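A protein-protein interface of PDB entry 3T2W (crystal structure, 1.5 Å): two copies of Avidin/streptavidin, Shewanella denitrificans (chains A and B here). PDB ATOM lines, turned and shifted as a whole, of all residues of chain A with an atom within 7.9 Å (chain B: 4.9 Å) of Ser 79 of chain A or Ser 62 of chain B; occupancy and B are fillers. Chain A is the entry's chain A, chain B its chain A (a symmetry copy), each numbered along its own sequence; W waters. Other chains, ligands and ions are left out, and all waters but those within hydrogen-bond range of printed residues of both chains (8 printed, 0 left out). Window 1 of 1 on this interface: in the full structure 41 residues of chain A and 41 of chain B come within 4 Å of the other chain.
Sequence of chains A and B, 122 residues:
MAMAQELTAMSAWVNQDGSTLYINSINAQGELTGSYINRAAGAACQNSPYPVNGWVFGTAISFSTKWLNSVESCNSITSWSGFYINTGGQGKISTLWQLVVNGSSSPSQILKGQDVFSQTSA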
ATOM      1  N   ASN A  53       0.677  14.409 -20.780  1.00  0.00           N
ATOM      2  CA  ASN A  53       1.737  14.895 -21.636  1.00  0.00           C
ATOM      3  C   ASN A  53       2.768  15.624 -20.762  1.00  0.00           C
ATOM      4  O   ASN A  53       2.568  15.754 -19.548  1.00  0.00           O
ATOM      5  CB  ASN A  53       1.203  15.742 -22.808  1.00  0.00           C
ATOM      6  CG  ASN A  53       0.391  16.925 -22.351  1.00  0.00           C
ATOM      7  OD1 ASN A  53       0.538  17.420 -21.239  1.00  0.00           O
ATOM      8  ND2 ASN A  53      -0.486  17.387 -23.226  1.00  0.00           N
ATOM      9  N   SER A  62       8.400  17.509 -16.316  1.00  0.00           N
ATOM     10  CA  SER A  62       7.051  18.015 -16.021  1.00  0.00           C
ATOM     11  C   SER A  62       6.050  17.069 -16.684  1.00  0.00           C
ATOM     12  O   SER A  62       6.330  16.463 -17.747  1.00  0.00           O
ATOM     13  CB  SER A  62       6.805  19.440 -16.530  1.00  0.00           C
ATOM     14  OG  SER A  62       6.600  19.445 -17.950  1.00  0.00           O
ATOM     15  N   PHE A  63       4.887  16.953 -16.069  1.00  0.00           N
ATOM     16  CA  PHE A  63       3.804  16.173 -16.675  1.00  0.00           C
ATOM     17  C   PHE A  63       2.459  16.701 -16.192  1.00  0.00           C
ATOM     18  O   PHE A  63       2.349  17.230 -15.085  1.00  0.00           O
ATOM     19  CB  PHE A  63       3.957  14.643 -16.473  1.00  0.00           C
ATOM     20  CG  PHE A  63       4.023  14.200 -15.023  1.00  0.00           C
ATOM     21  CD1 PHE A  63       5.221  14.205 -14.358  1.00  0.00           C
ATOM     22  CD2 PHE A  63       2.891  13.727 -14.370  1.00  0.00           C
ATOM     23  CE1 PHE A  63       5.306  13.788 -13.033  1.00  0.00           C
ATOM     24  CE2 PHE A  63       2.965  13.295 -13.032  1.00  0.00           C
ATOM     25  CZ  PHE A  63       4.193  13.313 -12.392  1.00  0.00           C
ATOM     26  N   SER A  64       1.431  16.603 -17.029  1.00  0.00           N
ATOM     27  CA  SER A  64       0.151  17.181 -16.741  1.00  0.00           C
ATOM     28  C   SER A  64      -0.947  16.286 -17.290  1.00  0.00           C
ATOM     29  O   SER A  64      -0.771  15.635 -18.339  1.00  0.00           O
ATOM     30  CB  SER A  64       0.067  18.578 -17.375  1.00  0.00           C
ATOM     31  OG  SER A  64      -1.202  19.193 -17.163  1.00  0.00           O
ATOM     32  N   THR A  65      -2.057  16.234 -16.567  1.00  0.00           N
ATOM     33  CA  THR A  65      -3.214  15.436 -17.009  1.00  0.00           C
ATOM     34  C   THR A  65      -4.496  16.238 -16.893  1.00  0.00           C
ATOM     35  O   THR A  65      -4.670  16.995 -15.928  1.00  0.00           O
ATOM     36  CB  THR A  65      -3.305  14.106 -16.209  1.00  0.00           C
ATOM     37  OG1 THR A  65      -4.273  13.254 -16.823  1.00  0.00           O
ATOM     38  CG2 THR A  65      -3.723  14.315 -14.761  1.00  0.00           C
ATOM     39  N   LYS A  66      -5.372  16.101 -17.896  1.00  0.00           N
ATOM     40  CA  LYS A  66      -6.737  16.605 -17.866  1.00  0.00           C
ATOM     41  C   LYS A  66      -7.639  15.505 -17.334  1.00  0.00           C
ATOM     42  O   LYS A  66      -7.624  14.384 -17.852  1.00  0.00           O
ATOM     43  CB  LYS A  66      -7.142  16.993 -19.287  1.00  0.00           C
ATOM     44  CG  LYS A  66      -8.631  17.305 -19.408  1.00  0.00           C
ATOM     45  CD  LYS A  66      -8.979  17.985 -20.729  1.00  0.00           C
ATOM     46  CE  LYS A  66     -10.489  18.086 -20.929  1.00  0.00           C
ATOM     47  NZ  LYS A  66     -10.819  18.772 -22.183  1.00  0.00           N
ATOM     48  N   TRP A  67      -8.406  15.811 -16.292  1.00  0.00           N
ATOM     49  CA  TRP A  67      -9.203  14.786 -15.626  1.00  0.00           C
ATOM     50  C   TRP A  67     -10.562  14.597 -16.320  1.00  0.00           C
ATOM     51  O   TRP A  67     -11.640  14.896 -15.767  1.00  0.00           O
ATOM     52  CB  TRP A  67      -9.376  15.163 -14.145  1.00  0.00           C
ATOM     53  CG  TRP A  67      -8.083  15.240 -13.383  1.00  0.00           C
ATOM     54  CD1 TRP A  67      -7.394  16.380 -13.001  1.00  0.00           C
ATOM     55  CD2 TRP A  67      -7.331  14.139 -12.898  1.00  0.00           C
ATOM     56  NE1 TRP A  67      -6.253  16.038 -12.302  1.00  0.00           N
ATOM     57  CE2 TRP A  67      -6.198  14.661 -12.229  1.00  0.00           C
ATOM     58  CE3 TRP A  67      -7.496  12.738 -12.970  1.00  0.00           C
ATOM     59  CZ2 TRP A  67      -5.242  13.836 -11.617  1.00  0.00           C
ATOM     60  CZ3 TRP A  67      -6.549  11.927 -12.347  1.00  0.00           C
ATOM     61  CH2 TRP A  67      -5.445  12.476 -11.672  1.00  0.00           C
ATOM     62  N   SER A  76     -11.081  19.453 -14.233  1.00  0.00           N
ATOM     63  CA  SER A  76      -9.860  19.994 -13.659  1.00  0.00           C
ATOM     64  C   SER A  76      -8.625  19.404 -14.370  1.00  0.00           C
ATOM     65  O   SER A  76      -8.711  18.445 -15.157  1.00  0.00           O
ATOM     66  CB  SER A  76      -9.806  19.624 -12.157  1.00  0.00           C
ATOM     67  OG  SER A  76      -9.699  18.216 -12.055  1.00  0.00           O
ATOM     68  N   ILE A  77      -7.488  20.031 -14.111  1.00  0.00           N
ATOM     69  CA  ILE A  77      -6.213  19.666 -14.701  1.00  0.00           C
ATOM     70  C   ILE A  77      -5.142  19.749 -13.625  1.00  0.00           C
ATOM     71  O   ILE A  77      -5.064  20.768 -12.915  1.00  0.00           O
ATOM     72  CB  ILE A  77      -5.801  20.663 -15.838  1.00  0.00           C
ATOM     73  CG1 ILE A  77      -6.859  20.742 -16.934  1.00  0.00           C
ATOM     74  CG2 ILE A  77      -4.443  20.302 -16.432  1.00  0.00           C
ATOM     75  CD1 ILE A  77      -6.694  21.970 -17.881  1.00  0.00           C
ATOM     76  N   THR A  78      -4.318  18.705 -13.499  1.00  0.00           N
ATOM     77  CA  THR A  78      -3.164  18.768 -12.598  1.00  0.00           C
ATOM     78  C   THR A  78      -1.884  18.873 -13.408  1.00  0.00           C
ATOM     79  O   THR A  78      -1.773  18.236 -14.456  1.00  0.00           O
ATOM     80  CB  THR A  78      -3.092  17.550 -11.667  1.00  0.00           C
ATOM     81  OG1 THR A  78      -4.306  17.534 -10.892  1.00  0.00           O
ATOM     82  CG2 THR A  78      -1.847  17.661 -10.766  1.00  0.00           C
ATOM     83  N   SER A  79      -0.932  19.660 -12.900  1.00  0.00           N
ATOM     84  CA  SER A  79       0.417  19.731 -13.441  1.00  0.00           C
ATOM     85  C   SER A  79       1.399  19.475 -12.352  1.00  0.00           C
ATOM     86  O   SER A  79       1.311  20.058 -11.263  1.00  0.00           O
ATOM     87  CB  SER A  79       0.691  21.147 -13.982  1.00  0.00           C
ATOM     88  OG  SER A  79      -0.201  21.361 -15.062  1.00  0.00           O
ATOM     89  N   TRP A  80       2.357  18.621 -12.660  1.00  0.00           N
ATOM     90  CA  TRP A  80       3.464  18.287 -11.762  1.00  0.00           C
ATOM     91  C   TRP A  80       4.763  18.823 -12.373  1.00  0.00           C
ATOM     92  O   TRP A  80       4.980  18.690 -13.568  1.00  0.00           O
ATOM     93  CB  TRP A  80       3.610  16.773 -11.598  1.00  0.00           C
ATOM     94  CG  TRP A  80       2.526  16.023 -10.841  1.00  0.00           C
ATOM     95  CD1 TRP A  80       2.575  15.578  -9.522  1.00  0.00           C
ATOM     96  CD2 TRP A  80       1.263  15.564 -11.356  1.00  0.00           C
ATOM     97  NE1 TRP A  80       1.434  14.874  -9.212  1.00  0.00           N
ATOM     98  CE2 TRP A  80       0.618  14.825 -10.314  1.00  0.00           C
ATOM     99  CE3 TRP A  80       0.646  15.622 -12.614  1.00  0.00           C
ATOM    100  CZ2 TRP A  80      -0.633  14.211 -10.491  1.00  0.00           C
ATOM    101  CZ3 TRP A  80      -0.584  15.004 -12.791  1.00  0.00           C
ATOM    102  CH2 TRP A  80      -1.215  14.285 -11.737  1.00  0.00           C
ATOM    103  N   SER A  81       5.640  19.369 -11.518  1.00  0.00           N
ATOM    104  CA  SER A  81       7.007  19.768 -11.879  1.00  0.00           C
ATOM    105  C   SER A  81       7.907  19.053 -10.910  1.00  0.00           C
ATOM    106  O   SER A  81       7.661  19.082  -9.692  1.00  0.00           O
ATOM    107  CB  SER A  81       7.209  21.277 -11.666  1.00  0.00           C
ATOM    108  OG  SER A  81       6.296  21.997 -12.491  1.00  0.00           O
ATOM    109  N   GLY A  82       8.944  18.421 -11.416  1.00  0.00           N
ATOM    110  CA  GLY A  82       9.801  17.681 -10.478  1.00  0.00           C
ATOM    111  C   GLY A  82      11.104  17.235 -11.049  1.00  0.00           C
ATOM    112  O   GLY A  82      11.499  17.634 -12.136  1.00  0.00           O
ATOM    113  N   THR A  95       8.199  15.816  -6.711  1.00  0.00           N
ATOM    114  CA  THR A  95       7.412  16.824  -7.469  1.00  0.00           C
ATOM    115  C   THR A  95       6.636  17.786  -6.589  1.00  0.00           C
ATOM    116  O   THR A  95       6.305  17.465  -5.415  1.00  0.00           O
ATOM    117  CB  THR A  95       6.339  16.157  -8.404  1.00  0.00           C
ATOM    118  OG1 THR A  95       5.252  15.649  -7.602  1.00  0.00           O
ATOM    119  CG2 THR A  95       6.941  15.053  -9.266  1.00  0.00           C
ATOM    120  N   LEU A  96       6.320  18.937  -7.185  1.00  0.00           N
ATOM    121  CA  LEU A  96       5.305  19.843  -6.691  1.00  0.00           C
ATOM    122  C   LEU A  96       4.221  19.898  -7.730  1.00  0.00           C
ATOM    123  O   LEU A  96       4.516  19.956  -8.933  1.00  0.00           O
ATOM    124  CB  LEU A  96       5.848  21.264  -6.462  1.00  0.00           C
ATOM    125  CG  LEU A  96       6.976  21.333  -5.436  1.00  0.00           C
ATOM    126  CD1 LEU A  96       7.496  22.752  -5.369  1.00  0.00           C
ATOM    127  CD2 LEU A  96       6.475  20.789  -4.064  1.00  0.00           C
ATOM    128  N   TRP A  97       2.984  19.852  -7.271  1.00  0.00           N
ATOM    129  CA  TRP A  97       1.837  19.897  -8.196  1.00  0.00           C
ATOM    130  C   TRP A  97       0.861  21.033  -7.960  1.00  0.00           C
ATOM    131  O   TRP A  97       0.785  21.596  -6.846  1.00  0.00           O
ATOM    132  CB  TRP A  97       1.101  18.538  -8.298  1.00  0.00           C
ATOM    133  CG  TRP A  97       0.565  17.992  -7.007  1.00  0.00           C
ATOM    134  CD1 TRP A  97       1.163  17.041  -6.237  1.00  0.00           C
ATOM    135  CD2 TRP A  97      -0.635  18.392  -6.319  1.00  0.00           C
ATOM    136  NE1 TRP A  97       0.393  16.785  -5.123  1.00  0.00           N
ATOM    137  CE2 TRP A  97      -0.720  17.581  -5.139  1.00  0.00           C
ATOM    138  CE3 TRP A  97      -1.677  19.293  -6.610  1.00  0.00           C
ATOM    139  CZ2 TRP A  97      -1.772  17.670  -4.249  1.00  0.00           C
ATOM    140  CZ3 TRP A  97      -2.741  19.384  -5.721  1.00  0.00           C
ATOM    141  CH2 TRP A  97      -2.764  18.574  -4.528  1.00  0.00           C
ATOM    142  N   GLN A  98       0.165  21.398  -9.017  1.00  0.00           N
ATOM    143  CA  GLN A  98      -0.858  22.411  -9.012  1.00  0.00           C
ATOM    144  C   GLN A  98      -2.080  21.841  -9.700  1.00  0.00           C
ATOM    145  O   GLN A  98      -1.972  21.269 -10.789  1.00  0.00           O
ATOM    146  CB  GLN A  98      -0.423  23.692  -9.752  1.00  0.00           C
ATOM    147  CG  GLN A  98       0.834  24.270  -9.203  1.00  0.00           C
ATOM    148  CD  GLN A  98       1.248  25.561  -9.900  1.00  0.00           C
ATOM    149  OE1 GLN A  98       1.130  25.705 -11.134  1.00  0.00           O
ATOM    150  NE2 GLN A  98       1.732  26.492  -9.115  1.00  0.00           N
ATOM    151  N   LEU A  99      -3.239  22.038  -9.101  1.00  0.00           N
ATOM    152  CA  LEU A  99      -4.501  21.553  -9.640  1.00  0.00           C
ATOM    153  C   LEU A  99      -5.431  22.739  -9.871  1.00  0.00           C
ATOM    154  O   LEU A  99      -5.790  23.466  -8.921  1.00  0.00           O
ATOM    155  CB  LEU A  99      -5.131  20.540  -8.662  1.00  0.00           C
ATOM    156  CG  LEU A  99      -6.526  19.934  -8.876  1.00  0.00           C
ATOM    157  CD1 LEU A  99      -7.683  20.833  -8.480  1.00  0.00           C
ATOM    158  CD2 LEU A  99      -6.732  19.360 -10.270  1.00  0.00           C
ATOM    159  N   VAL A 100      -5.805  22.962 -11.117  1.00  0.00           N
ATOM    160  CA  VAL A 100      -6.713  24.041 -11.452  1.00  0.00           C
ATOM    161  C   VAL A 100      -8.052  23.515 -11.988  1.00  0.00           C
ATOM    162  O   VAL A 100      -8.107  22.535 -12.747  1.00  0.00           O
ATOM    163  CB  VAL A 100      -6.044  25.038 -12.448  1.00  0.00           C
ATOM    164  CG1 VAL A 100      -5.724  24.372 -13.800  1.00  0.00           C
ATOM    165  CG2 VAL A 100      -6.912  26.276 -12.675  1.00  0.00           C
ATOM    166  N   LEU A 111      -5.205  24.441  -6.159  1.00  0.00           N
ATOM    167  CA  LEU A 111      -4.672  23.614  -5.077  1.00  0.00           C
ATOM    168  C   LEU A 111      -3.212  23.232  -5.335  1.00  0.00           C
ATOM    169  O   LEU A 111      -2.816  22.986  -6.481  1.00  0.00           O
ATOM    170  CB  LEU A 111      -5.545  22.361  -4.885  1.00  0.00           C
ATOM    171  CG  LEU A 111      -6.980  22.559  -4.347  1.00  0.00           C
ATOM    172  CD1 LEU A 111      -7.938  23.105  -5.389  1.00  0.00           C
ATOM    173  CD2 LEU A 111      -7.545  21.265  -3.770  1.00  0.00           C
ATOM    174  N   LYS A 112      -2.405  23.192  -4.295  1.00  0.00           N
ATOM    175  CA  LYS A 112      -1.010  22.871  -4.440  1.00  0.00           C
ATOM    176  C   LYS A 112      -0.713  21.760  -3.477  1.00  0.00           C
ATOM    177  O   LYS A 112      -1.366  21.652  -2.399  1.00  0.00           O
ATOM    178  CB  LYS A 112      -0.126  24.084  -4.111  1.00  0.00           C
ATOM    179  CG  LYS A 112      -0.327  25.333  -4.971  1.00  0.00           C
ATOM    180  CD  LYS A 112       0.623  26.413  -4.455  1.00  0.00           C
ATOM    181  CE  LYS A 112       0.566  27.677  -5.284  1.00  0.00           C
ATOM    182  NZ  LYS A 112      -0.326  28.709  -4.631  1.00  0.00           N
ATOM    183  N   GLY A 113       0.264  20.947  -3.837  1.00  0.00           N
ATOM    184  CA  GLY A 113       0.728  19.885  -2.979  1.00  0.00           C
ATOM    185  C   GLY A 113       2.055  19.329  -3.431  1.00  0.00           C
ATOM    186  O   GLY A 113       2.688  19.846  -4.369  1.00  0.00           O
ATOM    187  N   LEU B  32      -3.499  20.621 -25.995  1.00  0.00           N
ATOM    188  CA  LEU B  32      -2.975  21.868 -26.547  1.00  0.00           C
ATOM    189  C   LEU B  32      -1.577  21.697 -27.127  1.00  0.00           C
ATOM    190  O   LEU B  32      -0.745  20.982 -26.564  1.00  0.00           O
ATOM    191  CB  LEU B  32      -2.939  22.907 -25.398  1.00  0.00           C
ATOM    192  CG  LEU B  32      -2.351  24.296 -25.589  1.00  0.00           C
ATOM    193  CD1 LEU B  32      -3.075  25.310 -24.736  1.00  0.00           C
ATOM    194  CD2 LEU B  32      -0.843  24.355 -25.338  1.00  0.00           C
ATOM    195  N   ASN B  53       3.238  22.203 -24.765  1.00  0.00           N
ATOM    196  CA  ASN B  53       2.112  21.294 -24.778  1.00  0.00           C
ATOM    197  C   ASN B  53       1.239  21.588 -23.549  1.00  0.00           C
ATOM    198  O   ASN B  53       1.593  22.447 -22.732  1.00  0.00           O
ATOM    199  CB  ASN B  53       2.549  19.820 -24.894  1.00  0.00           C
ATOM    200  CG  ASN B  53       3.479  19.398 -23.788  1.00  0.00           C
ATOM    201  OD1 ASN B  53       3.497  19.972 -22.704  1.00  0.00           O
ATOM    202  ND2 ASN B  53       4.269  18.375 -24.065  1.00  0.00           N
ATOM    203  N   GLY B  54       0.104  20.922 -23.440  1.00  0.00           N
ATOM    204  CA  GLY B  54      -0.783  21.194 -22.309  1.00  0.00           C
ATOM    205  C   GLY B  54      -2.184  20.720 -22.560  1.00  0.00           C
ATOM    206  O   GLY B  54      -2.402  19.842 -23.395  1.00  0.00           O
ATOM    207  N   TRP B  55      -3.118  21.255 -21.780  1.00  0.00           N
ATOM    208  CA  TRP B  55      -4.514  20.847 -21.785  1.00  0.00           C
ATOM    209  C   TRP B  55      -5.404  22.069 -21.599  1.00  0.00           C
ATOM    210  O   TRP B  55      -5.023  23.020 -20.891  1.00  0.00           O
ATOM    211  CB  TRP B  55      -4.767  19.891 -20.585  1.00  0.00           C
ATOM    212  CG  TRP B  55      -4.058  18.590 -20.705  1.00  0.00           C
ATOM    213  CD1 TRP B  55      -2.960  18.203 -20.015  1.00  0.00           C
ATOM    214  CD2 TRP B  55      -4.392  17.501 -21.576  1.00  0.00           C
ATOM    215  NE1 TRP B  55      -2.567  16.930 -20.389  1.00  0.00           N
ATOM    216  CE2 TRP B  55      -3.436  16.479 -21.351  1.00  0.00           C
ATOM    217  CE3 TRP B  55      -5.426  17.275 -22.517  1.00  0.00           C
ATOM    218  CZ2 TRP B  55      -3.445  15.252 -22.056  1.00  0.00           C
ATOM    219  CZ3 TRP B  55      -5.442  16.038 -23.214  1.00  0.00           C
ATOM    220  CH2 TRP B  55      -4.461  15.052 -22.970  1.00  0.00           C
ATOM    221  N   ALA B  60     -10.299  26.221 -17.592  1.00  0.00           N
ATOM    222  CA  ALA B  60      -9.012  25.786 -17.018  1.00  0.00           C
ATOM    223  C   ALA B  60      -8.027  25.487 -18.141  1.00  0.00           C
ATOM    224  O   ALA B  60      -8.408  24.983 -19.200  1.00  0.00           O
ATOM    225  CB  ALA B  60      -9.156  24.535 -16.118  1.00  0.00           C
ATOM    226  N   ILE B  61      -6.763  25.791 -17.891  1.00  0.00           N
ATOM    227  CA  ILE B  61      -5.704  25.559 -18.895  1.00  0.00           C
ATOM    228  C   ILE B  61      -4.403  25.226 -18.173  1.00  0.00           C
ATOM    229  O   ILE B  61      -4.049  25.827 -17.138  1.00  0.00           O
ATOM    230  CB  ILE B  61      -5.557  26.748 -19.911  1.00  0.00           C
ATOM    231  CG1 ILE B  61      -4.420  26.456 -20.898  1.00  0.00           C
ATOM    232  CG2 ILE B  61      -5.303  28.091 -19.191  1.00  0.00           C
ATOM    233  CD1 ILE B  61      -4.336  27.476 -22.068  1.00  0.00           C
ATOM    234  N   SER B  62      -3.691  24.236 -18.680  1.00  0.00           N
ATOM    235  CA  SER B  62      -2.289  24.075 -18.267  1.00  0.00           C
ATOM    236  C   SER B  62      -1.433  24.081 -19.533  1.00  0.00           C
ATOM    237  O   SER B  62      -1.875  23.641 -20.622  1.00  0.00           O
ATOM    238  CB  SER B  62      -2.023  22.780 -17.491  1.00  0.00           C
ATOM    239  OG  SER B  62      -1.992  21.652 -18.378  1.00  0.00           O
ATOM    240  N   PHE B  63      -0.213  24.567 -19.390  1.00  0.00           N
ATOM    241  CA  PHE B  63       0.741  24.511 -20.502  1.00  0.00           C
ATOM    242  C   PHE B  63       2.163  24.483 -19.957  1.00  0.00           C
ATOM    243  O   PHE B  63       2.437  25.016 -18.881  1.00  0.00           O
ATOM    244  CB  PHE B  63       0.523  25.625 -21.559  1.00  0.00           C
ATOM    245  CG  PHE B  63       0.608  27.039 -21.014  1.00  0.00           C
ATOM    246  CD1 PHE B  63      -0.498  27.628 -20.459  1.00  0.00           C
ATOM    247  CD2 PHE B  63       1.780  27.776 -21.123  1.00  0.00           C
ATOM    248  CE1 PHE B  63      -0.447  28.928 -19.967  1.00  0.00           C
ATOM    249  CE2 PHE B  63       1.844  29.096 -20.637  1.00  0.00           C
ATOM    250  CZ  PHE B  63       0.705  29.659 -20.084  1.00  0.00           C
ATOM    251  N   SER B  64       3.075  23.828 -20.669  1.00  0.00           N
ATOM    252  CA  SER B  64       4.412  23.620 -20.195  1.00  0.00           C
ATOM    253  C   SER B  64       5.381  23.679 -21.365  1.00  0.00           C
ATOM    254  O   SER B  64       5.040  23.270 -22.493  1.00  0.00           O
ATOM    255  CB  SER B  64       4.500  22.254 -19.497  1.00  0.00           C
ATOM    256  OG  SER B  64       5.820  21.965 -19.040  1.00  0.00           O
ATOM    257  N   SER B  79       6.096  25.031 -16.043  1.00  0.00           N
ATOM    258  CA  SER B  79       4.698  24.643 -16.153  1.00  0.00           C
ATOM    259  C   SER B  79       3.842  25.713 -15.571  1.00  0.00           C
ATOM    260  O   SER B  79       4.096  26.199 -14.461  1.00  0.00           O
ATOM    261  CB  SER B  79       4.445  23.359 -15.341  1.00  0.00           C
ATOM    262  OG  SER B  79       5.210  22.328 -15.940  1.00  0.00           O
ATOM    263  N   TRP B  80       2.805  26.056 -16.311  1.00  0.00           N
ATOM    264  CA  TRP B  80       1.797  27.031 -15.892  1.00  0.00           C
ATOM    265  C   TRP B  80       0.468  26.298 -15.687  1.00  0.00           C
ATOM    266  O   TRP B  80       0.100  25.457 -16.494  1.00  0.00           O
ATOM    267  CB  TRP B  80       1.583  28.105 -16.960  1.00  0.00           C
ATOM    268  CG  TRP B  80       2.705  29.099 -17.218  1.00  0.00           C
ATOM    269  CD1 TRP B  80       2.790  30.410 -16.756  1.00  0.00           C
ATOM    270  CD2 TRP B  80       3.867  28.904 -18.044  1.00  0.00           C
ATOM    271  NE1 TRP B  80       3.917  31.021 -17.257  1.00  0.00           N
ATOM    272  CE2 TRP B  80       4.589  30.140 -18.066  1.00  0.00           C
ATOM    273  CE3 TRP B  80       4.330  27.847 -18.841  1.00  0.00           C
ATOM    274  CZ2 TRP B  80       5.771  30.307 -18.806  1.00  0.00           C
ATOM    275  CZ3 TRP B  80       5.490  28.018 -19.581  1.00  0.00           C
ATOM    276  CH2 TRP B  80       6.201  29.251 -19.578  1.00  0.00           C
ATOM    277  N   SER B  81      -0.265  26.681 -14.632  1.00  0.00           N
ATOM    278  CA  SER B  81      -1.640  26.232 -14.373  1.00  0.00           C
ATOM    279  C   SER B  81      -2.456  27.487 -14.234  1.00  0.00           C
ATOM    280  O   SER B  81      -2.063  28.408 -13.498  1.00  0.00           O
ATOM    281  CB  SER B  81      -1.725  25.477 -13.038  1.00  0.00           C
ATOM    282  OG  SER B  81      -0.879  24.332 -13.087  1.00  0.00           O
ATOM    283  N   GLN B  98       5.582  27.061 -12.181  1.00  0.00           N
ATOM    284  CA  GLN B  98       6.656  26.379 -11.509  1.00  0.00           C
ATOM    285  C   GLN B  98       7.751  26.120 -12.523  1.00  0.00           C
ATOM    286  O   GLN B  98       7.478  25.628 -13.621  1.00  0.00           O
ATOM    287  CB  GLN B  98       6.212  25.032 -10.903  1.00  0.00           C
ATOM    288  CG  GLN B  98       5.067  25.179  -9.964  1.00  0.00           C
ATOM    289  CD  GLN B  98       4.648  23.858  -9.327  1.00  0.00           C
ATOM    290  OE1 GLN B  98       4.623  22.795  -9.981  1.00  0.00           O
ATOM    291  NE2 GLN B  98       4.318  23.925  -8.060  1.00  0.00           N
HETATM  292  O   HOH W   1       2.137  19.457 -20.410  1.00  0.00           O
HETATM  293  O   HOH W   2       3.526  22.191 -12.200  1.00  0.00           O
HETATM  294  O   HOH W   3       2.926  23.211  -5.867  1.00  0.00           O
HETATM  295  O   HOH W   4      -2.519  22.409 -13.912  1.00  0.00           O
HETATM  296  O   HOH W   5       1.914  24.276 -13.093  1.00  0.00           O
HETATM  297  O   HOH W   6       3.517  20.196 -15.588  1.00  0.00           O
HETATM  298  O   HOH W   7       7.708  22.444 -14.699  1.00  0.00           O
HETATM  299  O   HOH W   8       1.394  22.856 -16.723  1.00  0.00           O
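O of Ser 64 of chain A lies within hydrogen-bond range of NE1 of Trp 55 of chain B, 3.0 Å away. The backbone carbonyl oxygen (O) of Gly 54 of chain B sits at hydrogen-bond distance from the side-chain amide nitrogen (ND2) of Asn 53 of chain A (3.1 Å). The backbone carbonyl oxygen (O) of Leu 96 of chain A sits close to the side-chain amide oxygen (OE1) of Gln 98 of chain B (3.0 Å). The side-chain hydroxyl (OG) of Ser 81 of chain B sits at hydrogen-bond distance from the side-chain amide oxygen (OE1) of Gln 98 of chain A, at 3.1 Å. OG of Ser 64 of chain A sits at hydrogen-bond distance from OG of Ser 62 of chain B (2.9 Å). The side-chain amide oxygen (OD1) of Asn 53 of chain A is in hydrogen-bond range of the indole nitrogen (NE1) of Trp 55 of chain B (3.3 Å). OG of Ser 81 of chain A sits at hydrogen-bond distance from OE1 of Gln 98 of chain B. The side-chain hydroxyl of Ser 62 of chain A is in hydrogen-bond range of the side-chain hydroxyl of Ser 64 of chain B (2.9 Å).
Ser 62 of chain A touches Ser 79 of chain B. O of Ala 60 of chain B touches CD1 of Ile 77 of chain A (3.7 Å). Ile 61 of chain B touches Ile 77 of chain A (N to CD1, 3.8 Å). Ile 77 of chain A touches Ser 62 of chain B (CG2 to OG, 3.4 Å). CB of Ser 62 of chain B touches OG of Ser 79 of chain A, 3.4 Å away. Gln 98 of chain B touches Gln 98 of chain A (NE2 to CG, 3.7 Å).
Water W4 lies within hydrogen-bond range of the side-chain hydroxyl (OG) of Ser 81 of chain B (2.7 Å), the side-chain hydroxyl (OG) of Ser 79 of chain A (2.8 Å), the backbone carbonyl oxygen (O) of Ile 77 of chain A (3.2 Å) and the backbone carbonyl oxygen (O) of Gln 98 of chain A (3.4 Å).
Printed residues of chain B that touch a printed residue of chain A: Gly 54, Trp 55, Ala 60, Ile 61, Ser 62, Ser 64, Ser 79, Ser 81 and Gln 98. Of the 23 printed residues of chain A, 10 touch a printed residue of chain B. Hydrophobic or aromatic side chains of chain A within 4 Å of the printed part of chain B: Ile 77 and Leu 96. Among the printed residues, no Asp or Glu carboxylate lies within 4 Å of a Lys or Arg side-chain nitrogen of the other chain.
Printed residues of chain B within 4 Å of Asn 53 of chain A: Gly 54 and Trp 55. Gly 82 of chain A touches none of the printed residues of chain B. Of the printed residues of chain A, Gly 54 of chain B touches Asn 53. Of the printed residues of chain A, Ala 60 of chain B touches Ile 77 (3.7 Å). Ser 62 of chain B touches three residues of chain A. The nearest residue of chain B that does not touch Ser 79 of chain A is Trp 80 of chain B (4.3 Å). The nearest printed residue of chain B that does not touch Asn 53 of chain A is Asn 53 of chain B (4.2 Å).
The backbone carbonyl oxygen of Asn 53 of chain B is in hydrogen-bond range of the backbone NH of Ser 64 of chain B (2.9 Å). The side-chain hydroxyl of Ser 64 of chain B is in hydrogen-bond range of the side-chain hydroxyl of Ser 79 of chain B, at 3.2 Å. N of Ser 79 of chain B lies within hydrogen-bond range of O of Gln 98 of chain B (2.9 Å). N of Ile 77 of chain A is in hydrogen-bond range of O of Val 100 of chain A.
Ser 79 of chain A touches Ser 81 of chain B, and with the chains exchanged Ser 81 of chain A touches Ser 79 of chain B. Ser 81 of chain A touches Gln 98 of chain B, and with the chains exchanged Gln 98 of chain A touches Ser 81 of chain B. Of the 19 pairs that touch across the chains among the printed residues, 9 have their exchanged pair printed and touching as well.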
